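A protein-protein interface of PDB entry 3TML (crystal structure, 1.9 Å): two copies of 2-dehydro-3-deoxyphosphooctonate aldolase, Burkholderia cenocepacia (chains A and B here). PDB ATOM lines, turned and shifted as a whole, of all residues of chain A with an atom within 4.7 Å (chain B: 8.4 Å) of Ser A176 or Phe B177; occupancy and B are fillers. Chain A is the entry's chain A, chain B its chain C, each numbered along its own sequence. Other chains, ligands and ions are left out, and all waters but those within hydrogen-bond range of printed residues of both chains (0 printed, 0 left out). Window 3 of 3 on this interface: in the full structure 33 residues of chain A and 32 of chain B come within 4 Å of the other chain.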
ATOM      1  N   GLN A 140     -13.160  -7.610  24.806  1.00  0.00           N
ATOM      2  CA  GLN A 140     -14.621  -7.526  24.704  1.00  0.00           C
ATOM      3  C   GLN A 140     -15.120  -6.446  23.744  1.00  0.00           C
ATOM      4  O   GLN A 140     -16.272  -6.449  23.351  1.00  0.00           O
ATOM      5  CB  GLN A 140     -15.224  -7.249  26.081  1.00  0.00           C
ATOM      6  CG  GLN A 140     -14.915  -8.356  27.095  1.00  0.00           C
ATOM      7  CD  GLN A 140     -13.649  -8.099  27.895  1.00  0.00           C
ATOM      8  OE1 GLN A 140     -12.711  -7.444  27.415  1.00  0.00           O
ATOM      9  NE2 GLN A 140     -13.618  -8.607  29.138  1.00  0.00           N
ATOM     10  N   GLY A 174     -15.772 -13.595  24.860  1.00  0.00           N
ATOM     11  CA  GLY A 174     -17.008 -12.828  24.879  1.00  0.00           C
ATOM     12  C   GLY A 174     -16.873 -11.433  24.298  1.00  0.00           C
ATOM     13  O   GLY A 174     -15.769 -10.818  24.293  1.00  0.00           O
ATOM     14  N   VAL A 175     -17.998 -10.921  23.783  1.00  0.00           N
ATOM     15  CA  VAL A 175     -18.062  -9.523  23.308  1.00  0.00           C
ATOM     16  C   VAL A 175     -19.161  -8.795  24.074  1.00  0.00           C
ATOM     17  O   VAL A 175     -20.153  -9.406  24.493  1.00  0.00           O
ATOM     18  CB  VAL A 175     -18.224  -9.419  21.758  1.00  0.00           C
ATOM     19  CG1 VAL A 175     -19.556 -10.025  21.272  1.00  0.00           C
ATOM     20  CG2 VAL A 175     -18.146  -7.973  21.284  1.00  0.00           C
ATOM     21  N   SER A 176     -18.946  -7.503  24.323  1.00  0.00           N
ATOM     22  CA  SER A 176     -19.925  -6.684  25.030  1.00  0.00           C
ATOM     23  C   SER A 176     -21.279  -6.753  24.320  1.00  0.00           C
ATOM     24  O   SER A 176     -21.349  -6.598  23.111  1.00  0.00           O
ATOM     25  CB  SER A 176     -19.460  -5.233  25.161  1.00  0.00           C
ATOM     26  OG  SER A 176     -18.318  -5.186  26.011  1.00  0.00           O
ATOM     27  N   PHE A 177     -22.333  -6.931  25.100  1.00  0.00           N
ATOM     28  CA  PHE A 177     -23.705  -6.994  24.589  1.00  0.00           C
ATOM     29  C   PHE A 177     -24.631  -6.161  25.488  1.00  0.00           C
ATOM     30  O   PHE A 177     -25.096  -6.633  26.524  1.00  0.00           O
ATOM     31  CB  PHE A 177     -24.180  -8.434  24.572  1.00  0.00           C
ATOM     32  CG  PHE A 177     -25.528  -8.630  23.934  1.00  0.00           C
ATOM     33  CD1 PHE A 177     -25.714  -8.339  22.616  1.00  0.00           C
ATOM     34  CD2 PHE A 177     -26.583  -9.152  24.652  1.00  0.00           C
ATOM     35  CE1 PHE A 177     -26.953  -8.520  22.012  1.00  0.00           C
ATOM     36  CE2 PHE A 177     -27.829  -9.354  24.058  1.00  0.00           C
ATOM     37  CZ  PHE A 177     -28.010  -9.035  22.746  1.00  0.00           C
ATOM     38  N   GLY A 178     -24.930  -4.940  25.064  1.00  0.00           N
ATOM     39  CA  GLY A 178     -25.546  -3.982  25.976  1.00  0.00           C
ATOM     40  C   GLY A 178     -24.683  -3.685  27.180  1.00  0.00           C
ATOM     41  O   GLY A 178     -23.458  -3.757  27.104  1.00  0.00           O
ATOM     42  N   ASN A 181     -23.367  -7.471  30.174  1.00  0.00           N
ATOM     43  CA  ASN A 181     -23.653  -8.757  29.565  1.00  0.00           C
ATOM     44  C   ASN A 181     -22.617  -8.964  28.475  1.00  0.00           C
ATOM     45  O   ASN A 181     -22.118  -7.982  27.875  1.00  0.00           O
ATOM     46  CB  ASN A 181     -25.082  -8.781  29.002  1.00  0.00           C
ATOM     47  CG  ASN A 181     -25.724 -10.205  28.963  1.00  0.00           C
ATOM     48  OD1 ASN A 181     -25.108 -11.196  29.251  1.00  0.00           O
ATOM     49  ND2 ASN A 181     -26.993 -10.256  28.643  1.00  0.00           N
ATOM     50  N   LEU A 182     -22.227 -10.216  28.263  1.00  0.00           N
ATOM     51  CA  LEU A 182     -21.398 -10.570  27.120  1.00  0.00           C
ATOM     52  C   LEU A 182     -22.164 -11.600  26.279  1.00  0.00           C
ATOM     53  O   LEU A 182     -22.962 -12.348  26.810  1.00  0.00           O
ATOM     54  CB  LEU A 182     -20.085 -11.210  27.545  1.00  0.00           C
ATOM     55  CG  LEU A 182     -19.077 -10.371  28.350  1.00  0.00           C
ATOM     56  CD1 LEU A 182     -17.982 -11.277  28.945  1.00  0.00           C
ATOM     57  CD2 LEU A 182     -18.453  -9.246  27.579  1.00  0.00           C
ATOM     58  N   VAL A 183     -21.905 -11.677  24.983  1.00  0.00           N
ATOM     59  CA  VAL A 183     -22.486 -12.735  24.204  1.00  0.00           C
ATOM     60  C   VAL A 183     -21.332 -13.449  23.493  1.00  0.00           C
ATOM     61  O   VAL A 183     -20.285 -12.843  23.228  1.00  0.00           O
ATOM     62  CB  VAL A 183     -23.504 -12.134  23.234  1.00  0.00           C
ATOM     63  CG1 VAL A 183     -22.799 -11.225  22.235  1.00  0.00           C
ATOM     64  CG2 VAL A 183     -24.301 -13.234  22.529  1.00  0.00           C
ATOM     65  N   GLN B 140     -36.506 -10.358  17.160  1.00  0.00           N
ATOM     66  CA  GLN B 140     -35.119  -9.944  17.259  1.00  0.00           C
ATOM     67  C   GLN B 140     -34.923  -8.995  18.451  1.00  0.00           C
ATOM     68  O   GLN B 140     -33.792  -8.753  18.900  1.00  0.00           O
ATOM     69  CB  GLN B 140     -34.653  -9.224  15.975  1.00  0.00           C
ATOM     70  CG  GLN B 140     -34.647 -10.113  14.743  1.00  0.00           C
ATOM     71  CD  GLN B 140     -35.997 -10.185  14.019  1.00  0.00           C
ATOM     72  OE1 GLN B 140     -37.089 -10.036  14.629  1.00  0.00           O
ATOM     73  NE2 GLN B 140     -35.932 -10.394  12.694  1.00  0.00           N
ATOM     74  N   GLY B 174     -32.175 -15.311  16.017  1.00  0.00           N
ATOM     75  CA  GLY B 174     -31.247 -14.240  16.209  1.00  0.00           C
ATOM     76  C   GLY B 174     -31.786 -13.122  17.083  1.00  0.00           C
ATOM     77  O   GLY B 174     -33.003 -12.879  17.137  1.00  0.00           O
ATOM     78  N   VAL B 175     -30.845 -12.348  17.663  1.00  0.00           N
ATOM     79  CA  VAL B 175     -31.177 -11.103  18.399  1.00  0.00           C
ATOM     80  C   VAL B 175     -30.343  -9.942  17.824  1.00  0.00           C
ATOM     81  O   VAL B 175     -29.197 -10.139  17.357  1.00  0.00           O
ATOM     82  CB  VAL B 175     -30.982 -11.309  19.911  1.00  0.00           C
ATOM     83  CG1 VAL B 175     -29.494 -11.402  20.282  1.00  0.00           C
ATOM     84  CG2 VAL B 175     -31.632 -10.222  20.770  1.00  0.00           C
ATOM     85  N   SER B 176     -30.925  -8.748  17.823  1.00  0.00           N
ATOM     86  CA  SER B 176     -30.287  -7.562  17.282  1.00  0.00           C
ATOM     87  C   SER B 176     -28.950  -7.311  18.012  1.00  0.00           C
ATOM     88  O   SER B 176     -28.900  -7.342  19.253  1.00  0.00           O
ATOM     89  CB  SER B 176     -31.199  -6.322  17.390  1.00  0.00           C
ATOM     90  OG  SER B 176     -32.411  -6.468  16.628  1.00  0.00           O
ATOM     91  N   PHE B 177     -27.906  -7.070  17.225  1.00  0.00           N
ATOM     92  CA  PHE B 177     -26.557  -6.816  17.739  1.00  0.00           C
ATOM     93  C   PHE B 177     -25.989  -5.594  17.060  1.00  0.00           C
ATOM     94  O   PHE B 177     -25.411  -5.687  16.004  1.00  0.00           O
ATOM     95  CB  PHE B 177     -25.672  -8.026  17.464  1.00  0.00           C
ATOM     96  CG  PHE B 177     -24.313  -7.929  18.103  1.00  0.00           C
ATOM     97  CD1 PHE B 177     -24.193  -7.777  19.481  1.00  0.00           C
ATOM     98  CD2 PHE B 177     -23.164  -7.965  17.340  1.00  0.00           C
ATOM     99  CE1 PHE B 177     -22.921  -7.655  20.073  1.00  0.00           C
ATOM    100  CE2 PHE B 177     -21.908  -7.853  17.928  1.00  0.00           C
ATOM    101  CZ  PHE B 177     -21.790  -7.704  19.298  1.00  0.00           C
ATOM    102  N   GLY B 178     -26.171  -4.436  17.665  1.00  0.00           N
ATOM    103  CA  GLY B 178     -25.876  -3.197  16.967  1.00  0.00           C
ATOM    104  C   GLY B 178     -26.783  -3.004  15.778  1.00  0.00           C
ATOM    105  O   GLY B 178     -27.932  -3.459  15.796  1.00  0.00           O
ATOM    106  N   TYR B 179     -26.271  -2.336  14.739  1.00  0.00           N
ATOM    107  CA  TYR B 179     -27.010  -2.104  13.499  1.00  0.00           C
ATOM    108  C   TYR B 179     -26.662  -3.141  12.437  1.00  0.00           C
ATOM    109  O   TYR B 179     -25.493  -3.475  12.279  1.00  0.00           O
ATOM    110  CB  TYR B 179     -26.665  -0.730  12.912  1.00  0.00           C
ATOM    111  CG  TYR B 179     -27.128   0.464  13.732  1.00  0.00           C
ATOM    112  CD1 TYR B 179     -28.381   0.487  14.312  1.00  0.00           C
ATOM    113  CD2 TYR B 179     -26.306   1.574  13.932  1.00  0.00           C
ATOM    114  CE1 TYR B 179     -28.804   1.585  15.072  1.00  0.00           C
ATOM    115  CE2 TYR B 179     -26.742   2.685  14.680  1.00  0.00           C
ATOM    116  CZ  TYR B 179     -27.998   2.667  15.257  1.00  0.00           C
ATOM    117  OH  TYR B 179     -28.463   3.718  16.003  1.00  0.00           O
ATOM    118  N   ASN B 180     -27.648  -3.602  11.692  1.00  0.00           N
ATOM    119  CA  ASN B 180     -27.402  -4.462  10.539  1.00  0.00           C
ATOM    120  C   ASN B 180     -26.668  -5.782  10.888  1.00  0.00           C
ATOM    121  O   ASN B 180     -25.878  -6.277  10.106  1.00  0.00           O
ATOM    122  CB  ASN B 180     -26.636  -3.669   9.475  1.00  0.00           C
ATOM    123  CG  ASN B 180     -27.359  -2.399   9.086  1.00  0.00           C
ATOM    124  OD1 ASN B 180     -26.808  -1.325   9.205  1.00  0.00           O
ATOM    125  ND2 ASN B 180     -28.620  -2.525   8.699  1.00  0.00           N
ATOM    126  N   ASN B 181     -26.957  -6.339  12.062  1.00  0.00           N
ATOM    127  CA  ASN B 181     -26.312  -7.563  12.497  1.00  0.00           C
ATOM    128  C   ASN B 181     -27.166  -8.253  13.534  1.00  0.00           C
ATOM    129  O   ASN B 181     -27.868  -7.600  14.329  1.00  0.00           O
ATOM    130  CB  ASN B 181     -24.895  -7.292  13.035  1.00  0.00           C
ATOM    131  CG  ASN B 181     -23.965  -8.503  12.882  1.00  0.00           C
ATOM    132  OD1 ASN B 181     -24.385  -9.584  12.510  1.00  0.00           O
ATOM    133  ND2 ASN B 181     -22.698  -8.296  13.119  1.00  0.00           N
ATOM    134  N   LEU B 182     -27.176  -9.573  13.458  1.00  0.00           N
ATOM    135  CA  LEU B 182     -27.867 -10.412  14.435  1.00  0.00           C
ATOM    136  C   LEU B 182     -26.797 -11.314  15.106  1.00  0.00           C
ATOM    137  O   LEU B 182     -25.872 -11.752  14.451  1.00  0.00           O
ATOM    138  CB  LEU B 182     -28.947 -11.291  13.808  1.00  0.00           C
ATOM    139  CG  LEU B 182     -30.197 -10.591  13.200  1.00  0.00           C
ATOM    140  CD1 LEU B 182     -31.159 -11.565  12.533  1.00  0.00           C
ATOM    141  CD2 LEU B 182     -30.980  -9.772  14.221  1.00  0.00           C
ATOM    142  N   VAL B 183     -26.928 -11.597  16.397  1.00  0.00           N
ATOM    143  CA  VAL B 183     -26.085 -12.593  17.023  1.00  0.00           C
ATOM    144  C   VAL B 183     -26.970 -13.747  17.517  1.00  0.00           C
ATOM    145  O   VAL B 183     -28.125 -13.532  17.894  1.00  0.00           O
ATOM    146  CB  VAL B 183     -25.205 -11.969  18.137  1.00  0.00           C
ATOM    147  CG1 VAL B 183     -26.055 -11.476  19.316  1.00  0.00           C
ATOM    148  CG2 VAL B 183     -24.113 -12.967  18.584  1.00  0.00           C
ATOM    149  N   SER B 184     -26.393 -14.958  17.500  1.00  0.00           N
ATOM    150  CA  SER B 184     -27.058 -16.152  17.943  1.00  0.00           C
ATOM    151  C   SER B 184     -26.514 -16.465  19.354  1.00  0.00           C
ATOM    152  O   SER B 184     -25.346 -16.982  19.539  1.00  0.00           O
ATOM    153  CB  SER B 184     -26.831 -17.297  16.913  1.00  0.00           C
ATOM    154  OG  SER B 184     -27.582 -18.439  17.285  1.00  0.00           O
ATOM    155  N   GLN B 208     -28.392 -13.743   9.020  1.00  0.00           N
ATOM    156  CA  GLN B 208     -28.689 -12.650   8.102  1.00  0.00           C
ATOM    157  C   GLN B 208     -28.193 -11.331   8.693  1.00  0.00           C
ATOM    158  O   GLN B 208     -28.067 -11.167   9.934  1.00  0.00           O
ATOM    159  CB  GLN B 208     -30.177 -12.601   7.726  1.00  0.00           C
ATOM    160  CG  GLN B 208     -31.039 -11.757   8.643  1.00  0.00           C
ATOM    161  CD  GLN B 208     -32.510 -12.088   8.494  1.00  0.00           C
ATOM    162  OE1 GLN B 208     -33.201 -12.272   9.477  1.00  0.00           O
ATOM    163  NE2 GLN B 208     -32.975 -12.221   7.262  1.00  0.00           N
ATOM    164  N   LEU B 209     -27.780 -10.437   7.804  1.00  0.00           N
ATOM    165  CA  LEU B 209     -27.424  -9.092   8.217  1.00  0.00           C
ATOM    166  C   LEU B 209     -28.602  -8.202   7.823  1.00  0.00           C
ATOM    167  O   LEU B 209     -28.740  -7.868   6.648  1.00  0.00           O
ATOM    168  CB  LEU B 209     -26.114  -8.643   7.554  1.00  0.00           C
ATOM    169  CG  LEU B 209     -24.879  -9.528   7.842  1.00  0.00           C
ATOM    170  CD1 LEU B 209     -23.651  -8.814   7.296  1.00  0.00           C
ATOM    171  CD2 LEU B 209     -24.672  -9.893   9.311  1.00  0.00           C
ATOM    172  N   PRO B 210     -29.465  -7.838   8.795  1.00  0.00           N
ATOM    173  CA  PRO B 210     -30.693  -7.062   8.478  1.00  0.00           C
ATOM    174  C   PRO B 210     -30.438  -5.787   7.691  1.00  0.00           C
ATOM    175  O   PRO B 210     -29.382  -5.172   7.819  1.00  0.00           O
ATOM    176  CB  PRO B 210     -31.244  -6.657   9.848  1.00  0.00           C
ATOM    177  CG  PRO B 210     -30.623  -7.570  10.831  1.00  0.00           C
ATOM    178  CD  PRO B 210     -29.360  -8.157  10.229  1.00  0.00           C
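The backbone carbonyl oxygen (O) of Gln A140 sits at hydrogen-bond distance from the backbone NH (N) of Ser A176 (3.0 Å).
The backbone carbonyl oxygen (O) of Val A175 lies within hydrogen-bond range of the backbone NH (N) of Val A183 (2.9 Å).
The backbone carbonyl oxygen of Gln B140 is in hydrogen-bond range of the backbone NH of Ser B176 (3.1 Å).
The backbone NH (N) of Val B183 is in hydrogen-bond range of the backbone carbonyl oxygen (O) of Val B175.
Among the printed residues, pairs that only touch across the chains: Phe A177 with Phe B177 (3.5 Å), Phe A177 with Ser B176 (3.6 Å), Ser A176 with Phe B177 (3.6 Å), Phe A177 with Val B175 (3.7 Å), Val A175 with Phe B177 (3.8 Å) and Val A183 with Val B183 (3.96 Å).
Val A175 touches one residue of chain B.
Printed residues of chain B within 4 Å of Phe A177: Val B175, Ser B176 and Phe B177.
Of the printed residues of chain A, Val B175 touches Phe A177.
Printed residues of chain A within 4 Å of Ser B176: Phe A177.
Of the printed residues of chain A, Val B183 touches Val A183 (3.96 Å).
The nearest residue of chain B that does not touch Ser A176 is Gly B178 (7.6 Å).
Printed residues of chain B that touch a printed residue of chain A: Val B175, Ser B176, Phe B177 and Val B183.
Hydrophobic or aromatic side chains of chain A that line the printed part of chain B: Val A175, Phe A177 and Val A183.
Among the printed residues, no Asp or Glu carboxylate lies within 4 Å of a Lys or Arg side-chain nitrogen of the other chain.
Val A175 touches Phe B177, and with the chains exchanged Phe A177 touches Val B175.
Ser A176 touches Phe B177, and with the chains exchanged Phe A177 touches Ser B176.
Phe B177 touches its own counterpart, Phe A177.
Val A183 touches its own counterpart, Val B183.
9 positions are printed for both chains.
Of the 6 pairs that touch across the chains among the printed residues, 6 have their exchanged pair printed and touching as well.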
